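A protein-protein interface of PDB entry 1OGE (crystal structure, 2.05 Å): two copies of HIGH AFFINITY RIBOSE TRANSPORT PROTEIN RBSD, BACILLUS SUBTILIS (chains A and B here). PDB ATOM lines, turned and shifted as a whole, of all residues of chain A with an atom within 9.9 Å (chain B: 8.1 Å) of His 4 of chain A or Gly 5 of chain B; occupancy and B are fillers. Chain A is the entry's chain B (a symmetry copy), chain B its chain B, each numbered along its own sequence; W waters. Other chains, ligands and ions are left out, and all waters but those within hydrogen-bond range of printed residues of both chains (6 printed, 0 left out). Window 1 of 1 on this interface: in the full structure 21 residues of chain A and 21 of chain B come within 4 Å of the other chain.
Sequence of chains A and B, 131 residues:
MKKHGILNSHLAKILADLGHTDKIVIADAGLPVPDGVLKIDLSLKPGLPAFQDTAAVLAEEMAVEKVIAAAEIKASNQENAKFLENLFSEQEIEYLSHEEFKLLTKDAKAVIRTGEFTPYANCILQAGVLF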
ATOM      1  N   MET A   1     -25.879   8.447  -6.863  1.00  0.00           N
ATOM      2  CA  MET A   1     -24.827   8.924  -5.924  1.00  0.00           C
ATOM      3  C   MET A   1     -23.429   8.732  -6.488  1.00  0.00           C
ATOM      4  O   MET A   1     -23.191   7.871  -7.337  1.00  0.00           O
ATOM      5  CB  MET A   1     -24.920   8.188  -4.587  1.00  0.00           C
ATOM      6  CG  MET A   1     -26.079   8.622  -3.703  1.00  0.00           C
ATOM      7  SD  MET A   1     -26.083   7.718  -2.141  1.00  0.00           S
ATOM      8  CE  MET A   1     -24.674   8.467  -1.292  1.00  0.00           C
ATOM      9  N   LYS A   2     -22.507   9.544  -5.993  1.00  0.00           N
ATOM     10  CA  LYS A   2     -21.114   9.506  -6.406  1.00  0.00           C
ATOM     11  C   LYS A   2     -20.464   8.258  -5.802  1.00  0.00           C
ATOM     12  O   LYS A   2     -20.500   8.055  -4.588  1.00  0.00           O
ATOM     13  CB  LYS A   2     -20.417  10.776  -5.908  1.00  0.00           C
ATOM     14  CG  LYS A   2     -19.003  10.977  -6.389  1.00  0.00           C
ATOM     15  CD  LYS A   2     -18.574  12.427  -6.178  1.00  0.00           C
ATOM     16  CE  LYS A   2     -18.452  12.784  -4.714  1.00  0.00           C
ATOM     17  NZ  LYS A   2     -17.233  12.204  -4.091  1.00  0.00           N
ATOM     18  N   LYS A   3     -19.876   7.425  -6.654  1.00  0.00           N
ATOM     19  CA  LYS A   3     -19.230   6.193  -6.199  1.00  0.00           C
ATOM     20  C   LYS A   3     -17.900   6.391  -5.489  1.00  0.00           C
ATOM     21  O   LYS A   3     -17.628   5.737  -4.482  1.00  0.00           O
ATOM     22  CB  LYS A   3     -18.992   5.242  -7.375  1.00  0.00           C
ATOM     23  CG  LYS A   3     -20.225   4.554  -7.906  1.00  0.00           C
ATOM     24  CD  LYS A   3     -19.840   3.601  -9.023  1.00  0.00           C
ATOM     25  CE  LYS A   3     -21.056   2.907  -9.606  1.00  0.00           C
ATOM     26  NZ  LYS A   3     -20.684   2.047 -10.761  1.00  0.00           N
ATOM     27  N   HIS A   4     -17.073   7.294  -6.004  1.00  0.00           N
ATOM     28  CA  HIS A   4     -15.751   7.504  -5.434  1.00  0.00           C
ATOM     29  C   HIS A   4     -15.467   8.898  -4.891  1.00  0.00           C
ATOM     30  O   HIS A   4     -16.220   9.844  -5.130  1.00  0.00           O
ATOM     31  CB  HIS A   4     -14.704   7.164  -6.494  1.00  0.00           C
ATOM     32  CG  HIS A   4     -14.957   5.863  -7.190  1.00  0.00           C
ATOM     33  ND1 HIS A   4     -14.980   5.746  -8.563  1.00  0.00           N
ATOM     34  CD2 HIS A   4     -15.215   4.627  -6.702  1.00  0.00           C
ATOM     35  CE1 HIS A   4     -15.245   4.494  -8.892  1.00  0.00           C
ATOM     36  NE2 HIS A   4     -15.392   3.795  -7.781  1.00  0.00           N
ATOM     37  N   GLY A   5     -14.357   8.997  -4.163  1.00  0.00           N
ATOM     38  CA  GLY A   5     -13.925  10.263  -3.600  1.00  0.00           C
ATOM     39  C   GLY A   5     -14.509  10.597  -2.245  1.00  0.00           C
ATOM     40  O   GLY A   5     -15.260   9.820  -1.660  1.00  0.00           O
ATOM     41  N   ILE A   6     -14.159  11.777  -1.752  1.00  0.00           N
ATOM     42  CA  ILE A   6     -14.626  12.247  -0.462  1.00  0.00           C
ATOM     43  C   ILE A   6     -16.157  12.316  -0.456  1.00  0.00           C
ATOM     44  O   ILE A   6     -16.788  12.659  -1.465  1.00  0.00           O
ATOM     45  CB  ILE A   6     -13.982  13.613  -0.150  1.00  0.00           C
ATOM     46  CG1 ILE A   6     -14.033  13.881   1.353  1.00  0.00           C
ATOM     47  CG2 ILE A   6     -14.671  14.710  -0.953  1.00  0.00           C
ATOM     48  CD1 ILE A   6     -12.997  14.888   1.816  1.00  0.00           C
ATOM     49  N   LEU A   7     -16.748  11.963   0.683  1.00  0.00           N
ATOM     50  CA  LEU A   7     -18.197  11.935   0.843  1.00  0.00           C
ATOM     51  C   LEU A   7     -18.866  13.300   0.966  1.00  0.00           C
ATOM     52  O   LEU A   7     -19.969  13.500   0.457  1.00  0.00           O
ATOM     53  CB  LEU A   7     -18.565  11.095   2.073  1.00  0.00           C
ATOM     54  CG  LEU A   7     -20.054  10.949   2.399  1.00  0.00           C
ATOM     55  CD1 LEU A   7     -20.759  10.183   1.291  1.00  0.00           C
ATOM     56  CD2 LEU A   7     -20.209  10.235   3.734  1.00  0.00           C
ATOM     57  N   ASN A   8     -18.214  14.232   1.649  1.00  0.00           N
ATOM     58  CA  ASN A   8     -18.797  15.557   1.836  1.00  0.00           C
ATOM     59  C   ASN A   8     -18.905  16.317   0.510  1.00  0.00           C
ATOM     60  O   ASN A   8     -17.908  16.506  -0.195  1.00  0.00           O
ATOM     61  CB  ASN A   8     -17.971  16.353   2.845  1.00  0.00           C
ATOM     62  CG  ASN A   8     -18.641  17.651   3.240  1.00  0.00           C
ATOM     63  OD1 ASN A   8     -18.638  18.625   2.474  1.00  0.00           O
ATOM     64  ND2 ASN A   8     -19.239  17.669   4.432  1.00  0.00           N
ATOM     65  N   SER A   9     -20.121  16.741   0.174  1.00  0.00           N
ATOM     66  CA  SER A   9     -20.356  17.454  -1.078  1.00  0.00           C
ATOM     67  C   SER A   9     -19.642  18.802  -1.158  1.00  0.00           C
ATOM     68  O   SER A   9     -19.103  19.150  -2.208  1.00  0.00           O
ATOM     69  CB  SER A   9     -21.861  17.633  -1.321  1.00  0.00           C
ATOM     70  OG  SER A   9     -22.467  18.360  -0.274  1.00  0.00           O
ATOM     71  N   ALA A  12     -15.957  18.037  -1.709  1.00  0.00           N
ATOM     72  CA  ALA A  12     -15.750  17.436  -3.027  1.00  0.00           C
ATOM     73  C   ALA A  12     -15.602  18.546  -4.072  1.00  0.00           C
ATOM     74  O   ALA A  12     -14.747  18.477  -4.957  1.00  0.00           O
ATOM     75  CB  ALA A  12     -16.928  16.525  -3.385  1.00  0.00           C
ATOM     76  N   LYS A  13     -16.431  19.579  -3.949  1.00  0.00           N
ATOM     77  CA  LYS A  13     -16.398  20.705  -4.883  1.00  0.00           C
ATOM     78  C   LYS A  13     -15.089  21.475  -4.818  1.00  0.00           C
ATOM     79  O   LYS A  13     -14.593  21.950  -5.834  1.00  0.00           O
ATOM     80  CB  LYS A  13     -17.575  21.644  -4.613  1.00  0.00           C
ATOM     81  CG  LYS A  13     -18.923  20.986  -4.847  1.00  0.00           C
ATOM     82  CD  LYS A  13     -20.069  21.905  -4.442  1.00  0.00           C
ATOM     83  CE  LYS A  13     -21.404  21.219  -4.641  1.00  0.00           C
ATOM     84  NZ  LYS A  13     -22.507  22.040  -4.090  1.00  0.00           N
ATOM     85  N   LEU A  15     -12.104  20.182  -3.687  1.00  0.00           N
ATOM     86  CA  LEU A  15     -11.020  19.322  -4.160  1.00  0.00           C
ATOM     87  C   LEU A  15     -11.023  19.267  -5.680  1.00  0.00           C
ATOM     88  O   LEU A  15      -9.969  19.247  -6.311  1.00  0.00           O
ATOM     89  CB  LEU A  15     -11.156  17.900  -3.593  1.00  0.00           C
ATOM     90  CG  LEU A  15     -10.958  17.760  -2.083  1.00  0.00           C
ATOM     91  CD1 LEU A  15     -11.036  16.290  -1.688  1.00  0.00           C
ATOM     92  CD2 LEU A  15      -9.615  18.348  -1.687  1.00  0.00           C
ATOM     93  N   ALA A  16     -12.220  19.255  -6.257  1.00  0.00           N
ATOM     94  CA  ALA A  16     -12.379  19.195  -7.702  1.00  0.00           C
ATOM     95  C   ALA A  16     -11.607  20.294  -8.436  1.00  0.00           C
ATOM     96  O   ALA A  16     -11.072  20.053  -9.518  1.00  0.00           O
ATOM     97  CB  ALA A  16     -13.849  19.264  -8.060  1.00  0.00           C
ATOM     98  N   GLU A  60      -6.207  11.164   2.517  1.00  0.00           N
ATOM     99  CA  GLU A  60      -6.570  10.029   1.683  1.00  0.00           C
ATOM    100  C   GLU A  60      -7.266  10.437   0.380  1.00  0.00           C
ATOM    101  O   GLU A  60      -7.294   9.672  -0.582  1.00  0.00           O
ATOM    102  CB  GLU A  60      -7.471   9.084   2.489  1.00  0.00           C
ATOM    103  CG  GLU A  60      -7.272   7.598   2.176  1.00  0.00           C
ATOM    104  CD  GLU A  60      -7.985   7.158   0.910  1.00  0.00           C
ATOM    105  OE1 GLU A  60      -7.680   6.051   0.406  1.00  0.00           O
ATOM    106  OE2 GLU A  60      -8.858   7.913   0.426  1.00  0.00           O
ATOM    107  N   GLU A  61      -7.807  11.650   0.335  1.00  0.00           N
ATOM    108  CA  GLU A  61      -8.521  12.091  -0.858  1.00  0.00           C
ATOM    109  C   GLU A  61      -7.825  13.175  -1.677  1.00  0.00           C
ATOM    110  O   GLU A  61      -8.239  13.477  -2.798  1.00  0.00           O
ATOM    111  CB  GLU A  61      -9.912  12.577  -0.461  1.00  0.00           C
ATOM    112  CG  GLU A  61     -10.797  11.509   0.157  1.00  0.00           C
ATOM    113  CD  GLU A  61     -11.019  10.315  -0.756  1.00  0.00           C
ATOM    114  OE1 GLU A  61     -10.828  10.445  -1.985  1.00  0.00           O
ATOM    115  OE2 GLU A  61     -11.401   9.241  -0.245  1.00  0.00           O
ATOM    116  N   MET A  62      -6.764  13.742  -1.120  1.00  0.00           N
ATOM    117  CA  MET A  62      -6.019  14.809  -1.770  1.00  0.00           C
ATOM    118  C   MET A  62      -4.523  14.516  -1.832  1.00  0.00           C
ATOM    119  O   MET A  62      -3.942  14.028  -0.867  1.00  0.00           O
ATOM    120  CB  MET A  62      -6.257  16.107  -0.989  1.00  0.00           C
ATOM    121  CG  MET A  62      -5.377  17.279  -1.357  1.00  0.00           C
ATOM    122  SD  MET A  62      -5.609  18.613  -0.154  1.00  0.00           S
ATOM    123  CE  MET A  62      -4.461  19.839  -0.786  1.00  0.00           C
ATOM    124  N   LEU A 130      -0.654  14.885  -9.778  1.00  0.00           N
ATOM    125  CA  LEU A 130      -0.802  13.448 -10.003  1.00  0.00           C
ATOM    126  C   LEU A 130       0.117  12.899 -11.097  1.00  0.00           C
ATOM    127  O   LEU A 130       0.087  11.707 -11.402  1.00  0.00           O
ATOM    128  CB  LEU A 130      -2.253  13.109 -10.352  1.00  0.00           C
ATOM    129  CG  LEU A 130      -3.272  13.286  -9.226  1.00  0.00           C
ATOM    130  CD1 LEU A 130      -4.652  12.872  -9.712  1.00  0.00           C
ATOM    131  CD2 LEU A 130      -2.854  12.447  -8.022  1.00  0.00           C
ATOM    132  N   LYS B   2      -7.186  16.239  -6.550  1.00  0.00           N
ATOM    133  CA  LYS B   2      -8.118  15.226  -6.085  1.00  0.00           C
ATOM    134  C   LYS B   2      -7.620  13.857  -6.557  1.00  0.00           C
ATOM    135  O   LYS B   2      -7.401  13.645  -7.751  1.00  0.00           O
ATOM    136  CB  LYS B   2      -9.504  15.527  -6.661  1.00  0.00           C
ATOM    137  CG  LYS B   2     -10.628  14.665  -6.146  1.00  0.00           C
ATOM    138  CD  LYS B   2     -11.976  15.308  -6.462  1.00  0.00           C
ATOM    139  CE  LYS B   2     -12.267  15.336  -7.946  1.00  0.00           C
ATOM    140  NZ  LYS B   2     -12.644  13.998  -8.473  1.00  0.00           N
ATOM    141  N   LYS B   3      -7.438  12.936  -5.617  1.00  0.00           N
ATOM    142  CA  LYS B   3      -6.954  11.593  -5.943  1.00  0.00           C
ATOM    143  C   LYS B   3      -7.975  10.690  -6.618  1.00  0.00           C
ATOM    144  O   LYS B   3      -7.641   9.966  -7.555  1.00  0.00           O
ATOM    145  CB  LYS B   3      -6.460  10.876  -4.683  1.00  0.00           C
ATOM    146  CG  LYS B   3      -5.139  11.363  -4.142  1.00  0.00           C
ATOM    147  CD  LYS B   3      -4.741  10.532  -2.936  1.00  0.00           C
ATOM    148  CE  LYS B   3      -3.429  11.007  -2.342  1.00  0.00           C
ATOM    149  NZ  LYS B   3      -3.091  10.251  -1.106  1.00  0.00           N
ATOM    150  N   HIS B   4      -9.217  10.734  -6.151  1.00  0.00           N
ATOM    151  CA  HIS B   4     -10.246   9.857  -6.686  1.00  0.00           C
ATOM    152  C   HIS B   4     -11.442  10.541  -7.334  1.00  0.00           C
ATOM    153  O   HIS B   4     -11.636  11.752  -7.203  1.00  0.00           O
ATOM    154  CB  HIS B   4     -10.745   8.947  -5.565  1.00  0.00           C
ATOM    155  CG  HIS B   4      -9.644   8.316  -4.772  1.00  0.00           C
ATOM    156  ND1 HIS B   4      -9.593   8.369  -3.395  1.00  0.00           N
ATOM    157  CD2 HIS B   4      -8.544   7.632  -5.163  1.00  0.00           C
ATOM    158  CE1 HIS B   4      -8.506   7.748  -2.972  1.00  0.00           C
ATOM    159  NE2 HIS B   4      -7.852   7.292  -4.026  1.00  0.00           N
ATOM    160  N   GLY B   5     -12.241   9.732  -8.027  1.00  0.00           N
ATOM    161  CA  GLY B   5     -13.443  10.220  -8.677  1.00  0.00           C
ATOM    162  C   GLY B   5     -13.242  10.761 -10.077  1.00  0.00           C
ATOM    163  O   GLY B   5     -12.142  10.740 -10.621  1.00  0.00           O
ATOM    164  N   ILE B   6     -14.328  11.257 -10.653  1.00  0.00           N
ATOM    165  CA  ILE B   6     -14.309  11.808 -11.994  1.00  0.00           C
ATOM    166  C   ILE B   6     -13.322  12.979 -12.062  1.00  0.00           C
ATOM    167  O   ILE B   6     -13.183  13.757 -11.109  1.00  0.00           O
ATOM    168  CB  ILE B   6     -15.737  12.229 -12.396  1.00  0.00           C
ATOM    169  CG1 ILE B   6     -15.845  12.321 -13.917  1.00  0.00           C
ATOM    170  CG2 ILE B   6     -16.106  13.541 -11.714  1.00  0.00           C
ATOM    171  CD1 ILE B   6     -17.269  12.200 -14.424  1.00  0.00           C
ATOM    172  N   LEU B   7     -12.621  13.079 -13.189  1.00  0.00           N
ATOM    173  CA  LEU B   7     -11.612  14.111 -13.399  1.00  0.00           C
ATOM    174  C   LEU B   7     -12.157  15.511 -13.660  1.00  0.00           C
ATOM    175  O   LEU B   7     -11.574  16.499 -13.212  1.00  0.00           O
ATOM    176  CB  LEU B   7     -10.700  13.713 -14.567  1.00  0.00           C
ATOM    177  CG  LEU B   7      -9.572  14.680 -14.934  1.00  0.00           C
ATOM    178  CD1 LEU B   7      -8.572  14.775 -13.793  1.00  0.00           C
ATOM    179  CD2 LEU B   7      -8.893  14.202 -16.209  1.00  0.00           C
ATOM    180  N   ASN B   8     -13.258  15.603 -14.395  1.00  0.00           N
ATOM    181  CA  ASN B   8     -13.829  16.908 -14.713  1.00  0.00           C
ATOM    182  C   ASN B   8     -14.363  17.611 -13.461  1.00  0.00           C
ATOM    183  O   ASN B   8     -15.203  17.064 -12.738  1.00  0.00           O
ATOM    184  CB  ASN B   8     -14.936  16.752 -15.755  1.00  0.00           C
ATOM    185  CG  ASN B   8     -15.421  18.085 -16.282  1.00  0.00           C
ATOM    186  OD1 ASN B   8     -16.166  18.804 -15.601  1.00  0.00           O
ATOM    187  ND2 ASN B   8     -14.985  18.438 -17.493  1.00  0.00           N
ATOM    188  N   ALA B  12     -17.705  16.790 -11.287  1.00  0.00           N
ATOM    189  CA  ALA B  12     -17.453  16.344  -9.916  1.00  0.00           C
ATOM    190  C   ALA B  12     -18.407  17.071  -8.964  1.00  0.00           C
ATOM    191  O   ALA B  12     -18.969  16.470  -8.045  1.00  0.00           O
ATOM    192  CB  ALA B  12     -15.999  16.625  -9.527  1.00  0.00           C
ATOM    193  N   LEU B  15     -21.965  15.570  -9.356  1.00  0.00           N
ATOM    194  CA  LEU B  15     -22.085  14.235  -8.772  1.00  0.00           C
ATOM    195  C   LEU B  15     -22.098  14.328  -7.255  1.00  0.00           C
ATOM    196  O   LEU B  15     -22.821  13.593  -6.585  1.00  0.00           O
ATOM    197  CB  LEU B  15     -20.928  13.330  -9.223  1.00  0.00           C
ATOM    198  CG  LEU B  15     -20.904  12.963 -10.707  1.00  0.00           C
ATOM    199  CD1 LEU B  15     -19.757  11.998 -10.980  1.00  0.00           C
ATOM    200  CD2 LEU B  15     -22.231  12.340 -11.102  1.00  0.00           C
ATOM    201  N   ALA B  16     -21.300  15.247  -6.723  1.00  0.00           N
ATOM    202  CA  ALA B  16     -21.202  15.445  -5.285  1.00  0.00           C
ATOM    203  C   ALA B  16     -22.558  15.680  -4.618  1.00  0.00           C
ATOM    204  O   ALA B  16     -22.784  15.215  -3.500  1.00  0.00           O
ATOM    205  CB  ALA B  16     -20.269  16.600  -4.989  1.00  0.00           C
ATOM    206  N   VAL B  57     -17.644   6.812 -18.833  1.00  0.00           N
ATOM    207  CA  VAL B  57     -17.027   7.440 -17.676  1.00  0.00           C
ATOM    208  C   VAL B  57     -18.067   7.664 -16.571  1.00  0.00           C
ATOM    209  O   VAL B  57     -17.812   7.384 -15.400  1.00  0.00           O
ATOM    210  CB  VAL B  57     -16.375   8.787 -18.058  1.00  0.00           C
ATOM    211  CG1 VAL B  57     -15.863   9.492 -16.806  1.00  0.00           C
ATOM    212  CG2 VAL B  57     -15.222   8.546 -19.040  1.00  0.00           C
ATOM    213  N   ALA B  59     -20.918   6.062 -16.002  1.00  0.00           N
ATOM    214  CA  ALA B  59     -21.361   4.797 -15.438  1.00  0.00           C
ATOM    215  C   ALA B  59     -20.377   4.295 -14.385  1.00  0.00           C
ATOM    216  O   ALA B  59     -20.756   3.610 -13.432  1.00  0.00           O
ATOM    217  CB  ALA B  59     -21.508   3.761 -16.548  1.00  0.00           C
ATOM    218  N   GLU B  60     -19.110   4.645 -14.560  1.00  0.00           N
ATOM    219  CA  GLU B  60     -18.061   4.218 -13.647  1.00  0.00           C
ATOM    220  C   GLU B  60     -17.937   5.114 -12.410  1.00  0.00           C
ATOM    221  O   GLU B  60     -17.392   4.699 -11.389  1.00  0.00           O
ATOM    222  CB  GLU B  60     -16.726   4.175 -14.404  1.00  0.00           C
ATOM    223  CG  GLU B  60     -15.782   3.055 -13.960  1.00  0.00           C
ATOM    224  CD  GLU B  60     -15.022   3.388 -12.689  1.00  0.00           C
ATOM    225  OE1 GLU B  60     -14.434   2.462 -12.083  1.00  0.00           O
ATOM    226  OE2 GLU B  60     -15.003   4.579 -12.303  1.00  0.00           O
ATOM    227  N   GLU B  61     -18.463   6.331 -12.487  1.00  0.00           N
ATOM    228  CA  GLU B  61     -18.347   7.252 -11.362  1.00  0.00           C
ATOM    229  C   GLU B  61     -19.645   7.541 -10.612  1.00  0.00           C
ATOM    230  O   GLU B  61     -19.627   8.142  -9.537  1.00  0.00           O
ATOM    231  CB  GLU B  61     -17.746   8.568 -11.849  1.00  0.00           C
ATOM    232  CG  GLU B  61     -16.339   8.447 -12.408  1.00  0.00           C
ATOM    233  CD  GLU B  61     -15.346   7.883 -11.407  1.00  0.00           C
ATOM    234  OE1 GLU B  61     -15.616   7.933 -10.187  1.00  0.00           O
ATOM    235  OE2 GLU B  61     -14.279   7.397 -11.840  1.00  0.00           O
ATOM    236  N   MET B  62     -20.760   7.096 -11.176  1.00  0.00           N
ATOM    237  CA  MET B  62     -22.072   7.322 -10.590  1.00  0.00           C
ATOM    238  C   MET B  62     -22.873   6.031 -10.449  1.00  0.00           C
ATOM    239  O   MET B  62     -22.872   5.195 -11.347  1.00  0.00           O
ATOM    240  CB  MET B  62     -22.836   8.306 -11.485  1.00  0.00           C
ATOM    241  CG  MET B  62     -24.306   8.479 -11.184  1.00  0.00           C
ATOM    242  SD  MET B  62     -25.084   9.448 -12.503  1.00  0.00           S
ATOM    243  CE  MET B  62     -26.785   9.483 -11.935  1.00  0.00           C
ATOM    244  N   ALA B  63     -23.548   5.866  -9.317  1.00  0.00           N
ATOM    245  CA  ALA B  63     -24.381   4.688  -9.103  1.00  0.00           C
ATOM    246  C   ALA B  63     -25.709   4.961  -9.804  1.00  0.00           C
ATOM    247  O   ALA B  63     -26.474   5.829  -9.388  1.00  0.00           O
ATOM    248  CB  ALA B  63     -24.608   4.460  -7.620  1.00  0.00           C
ATOM    249  N   LEU B 130     -26.059   4.105  -2.425  1.00  0.00           N
ATOM    250  CA  LEU B 130     -24.911   3.265  -2.086  1.00  0.00           C
ATOM    251  C   LEU B 130     -25.171   2.312  -0.916  1.00  0.00           C
ATOM    252  O   LEU B 130     -24.286   1.557  -0.514  1.00  0.00           O
ATOM    253  CB  LEU B 130     -23.691   4.131  -1.763  1.00  0.00           C
ATOM    254  CG  LEU B 130     -23.089   4.905  -2.937  1.00  0.00           C
ATOM    255  CD1 LEU B 130     -21.868   5.680  -2.468  1.00  0.00           C
ATOM    256  CD2 LEU B 130     -22.712   3.931  -4.049  1.00  0.00           C
HETATM  257  O   HOH W   1     -11.724  17.412 -10.407  1.00  0.00           O
HETATM  258  O   HOH W   2     -17.394   8.882  -8.325  1.00  0.00           O
HETATM  259  O   HOH W   3      -8.128  18.470  -8.341  1.00  0.00           O
HETATM  260  O   HOH W   4     -10.252  12.234  -3.984  1.00  0.00           O
HETATM  261  O   HOH W   5     -23.573  11.888  -4.431  1.00  0.00           O
HETATM  262  O   HOH W   6     -20.435  13.990  -2.417  1.00  0.00           O
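A ring nitrogen (ND1) of His 4 of chain A is in hydrogen-bond range of the side-chain carboxylate (OE1) of Glu 61 of chain B (2.8 Å). ND1 of His 4 of chain B is in hydrogen-bond range of OE1 of Glu 61 of chain A. The backbone NH (N) of Leu 130 of chain B lies within hydrogen-bond range of the side-chain sulfur (SD) of Met 1 of chain A, 3.6 Å away. O of Ala 59 of chain B sits at hydrogen-bond distance from NZ of Lys 3 of chain A (3.1 Å). N of Lys 3 of chain A lies within hydrogen-bond range of O of Glu 61 of chain B (3.0 Å). The backbone carbonyl oxygen of Met 1 of chain A sits at hydrogen-bond distance from the backbone NH of Ala 63 of chain B, at 2.8 Å. O of Glu 61 of chain A lies within hydrogen-bond range of N of Lys 3 of chain B (3.0 Å).
NZ of Lys 2 of chain A sits at hydrogen-bond distance from O of His 4 of chain A (2.8 Å). The side-chain amino group of Lys 2 of chain B lies within hydrogen-bond range of the backbone carbonyl oxygen of Ile 6 of chain B (2.7 Å). The side-chain amino group (NZ) of Lys 2 of chain B is in hydrogen-bond range of the backbone carbonyl oxygen (O) of His 4 of chain B (2.8 Å). NZ of Lys 2 of chain A sits at hydrogen-bond distance from O of Ile 6 of chain A (2.7 Å).
Lys 2 of chain A touches Glu 61 of chain B (CA to O, 3.7 Å). Lys 2 of chain A touches Leu 130 of chain B (O to CD1, 3.5 Å). O of Glu 60 of chain B touches CD of Lys 3 of chain A, 3.6 Å away. His 4 of chain A touches Glu 60 of chain B. His 4 of chain B touches Gly 5 of chain A (CB to N, 3.9 Å). Ser 9 of chain A touches Ala 16 of chain B (CB to O, 3.4 Å). CA of Ala 16 of chain A touches CE of Lys 2 of chain B, 3.9 Å away. CA of Lys 2 of chain B touches O of Glu 61 of chain A, at 3.7 Å. Met 62 of chain A touches Lys 3 of chain B (O to CE, 3.4 Å). Lys 2 of chain B touches Leu 130 of chain A.
His 4 of chain A touches just these residues of chain B: Gly 5 (3.9 Å), Glu 60 (3.3 Å) and Glu 61 (2.8 Å). Asn 8 of chain A touches none of the printed residues of chain B. Of the printed residues of chain B, Glu 60 of chain A touches Lys 3 and His 4. Of the printed residues of chain B, Leu 130 of chain A touches Lys 2 (3.5 Å). Of the printed residues of chain A, His 4 of chain B touches Gly 5 (3.9 Å), Glu 60 (3.3 Å) and Glu 61 (2.8 Å). Gly 5 of chain B touches just one residue of chain A: His 4. Leu 7 of chain B touches none of the printed residues of chain A. Of the printed residues of chain A, Ala 59 of chain B touches Lys 3. Glu 61 of chain B touches just these residues of chain A: Lys 2 (3.7 Å), Lys 3 (3.0 Å) and His 4 (2.8 Å). Printed residues of chain A within 4 Å of Ala 63 of chain B: Met 1 and Lys 3. The nearest residue of chain B that does not touch His 4 of chain A is His 4 of chain B (4.4 Å). The nearest printed residue of chain A that does not touch Ala 59 of chain B is His 4 of chain A (7.2 Å).
Of the 17 printed residues of chain B, 13 touch a printed residue of chain A. Hydrophobic or aromatic side chains of chain B within 4 Å of the printed part of chain A: His 4, Ala 12, Leu 15, Ala 16, Ala 63 and Leu 130. Among the printed residues, 28 pairs touch across the chains. Among the printed residues, no Asp or Glu carboxylate lies within 4 Å of a Lys or Arg side-chain nitrogen of the other chain.
Lys 2 of chain A touches Leu 15 of chain B, and with the chains exchanged Leu 15 of chain A touches Lys 2 of chain B. Lys 2 of chain A touches Glu 61 of chain B, and with the chains exchanged Glu 61 of chain A touches Lys 2 of chain B. Lys 3 of chain A touches Glu 61 of chain B, and with the chains exchanged Glu 61 of chain A touches Lys 3 of chain B. Ala 12 of chain A touches Ala 16 of chain B, and with the chains exchanged Ala 16 of chain A touches Ala 12 of chain B. 14 positions are printed for both chains.
Water W2 lies within hydrogen-bond range of O of Glu 61 of chain B (2.6 Å), N of His 4 of chain A (2.8 Å) and N of Lys 3 of chain A (3.3 Å). Water W4 lies within hydrogen-bond range of the backbone carbonyl oxygen (O) of Glu 61 of chain A (2.6 Å), the backbone NH (N) of His 4 of chain B (2.8 Å) and the backbone NH (N) of Lys 3 of chain B (3.3 Å). Water W5 bridges the backbone carbonyl oxygen of Leu 15 of chain B and the backbone NH of Lys 2 of chain A. Water W3 lies within hydrogen-bond range of O of Leu 15 of chain A (2.8 Å) and N of Lys 2 of chain B (3.0 Å). Water W1 bridges O of Ala 16 of chain A (2.9 Å) and O of Leu 7 of chain B (3.0 Å). Water W6 bridges O of Ala 16 of chain B (2.9 Å) and O of Leu 7 of chain A (3.0 Å).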
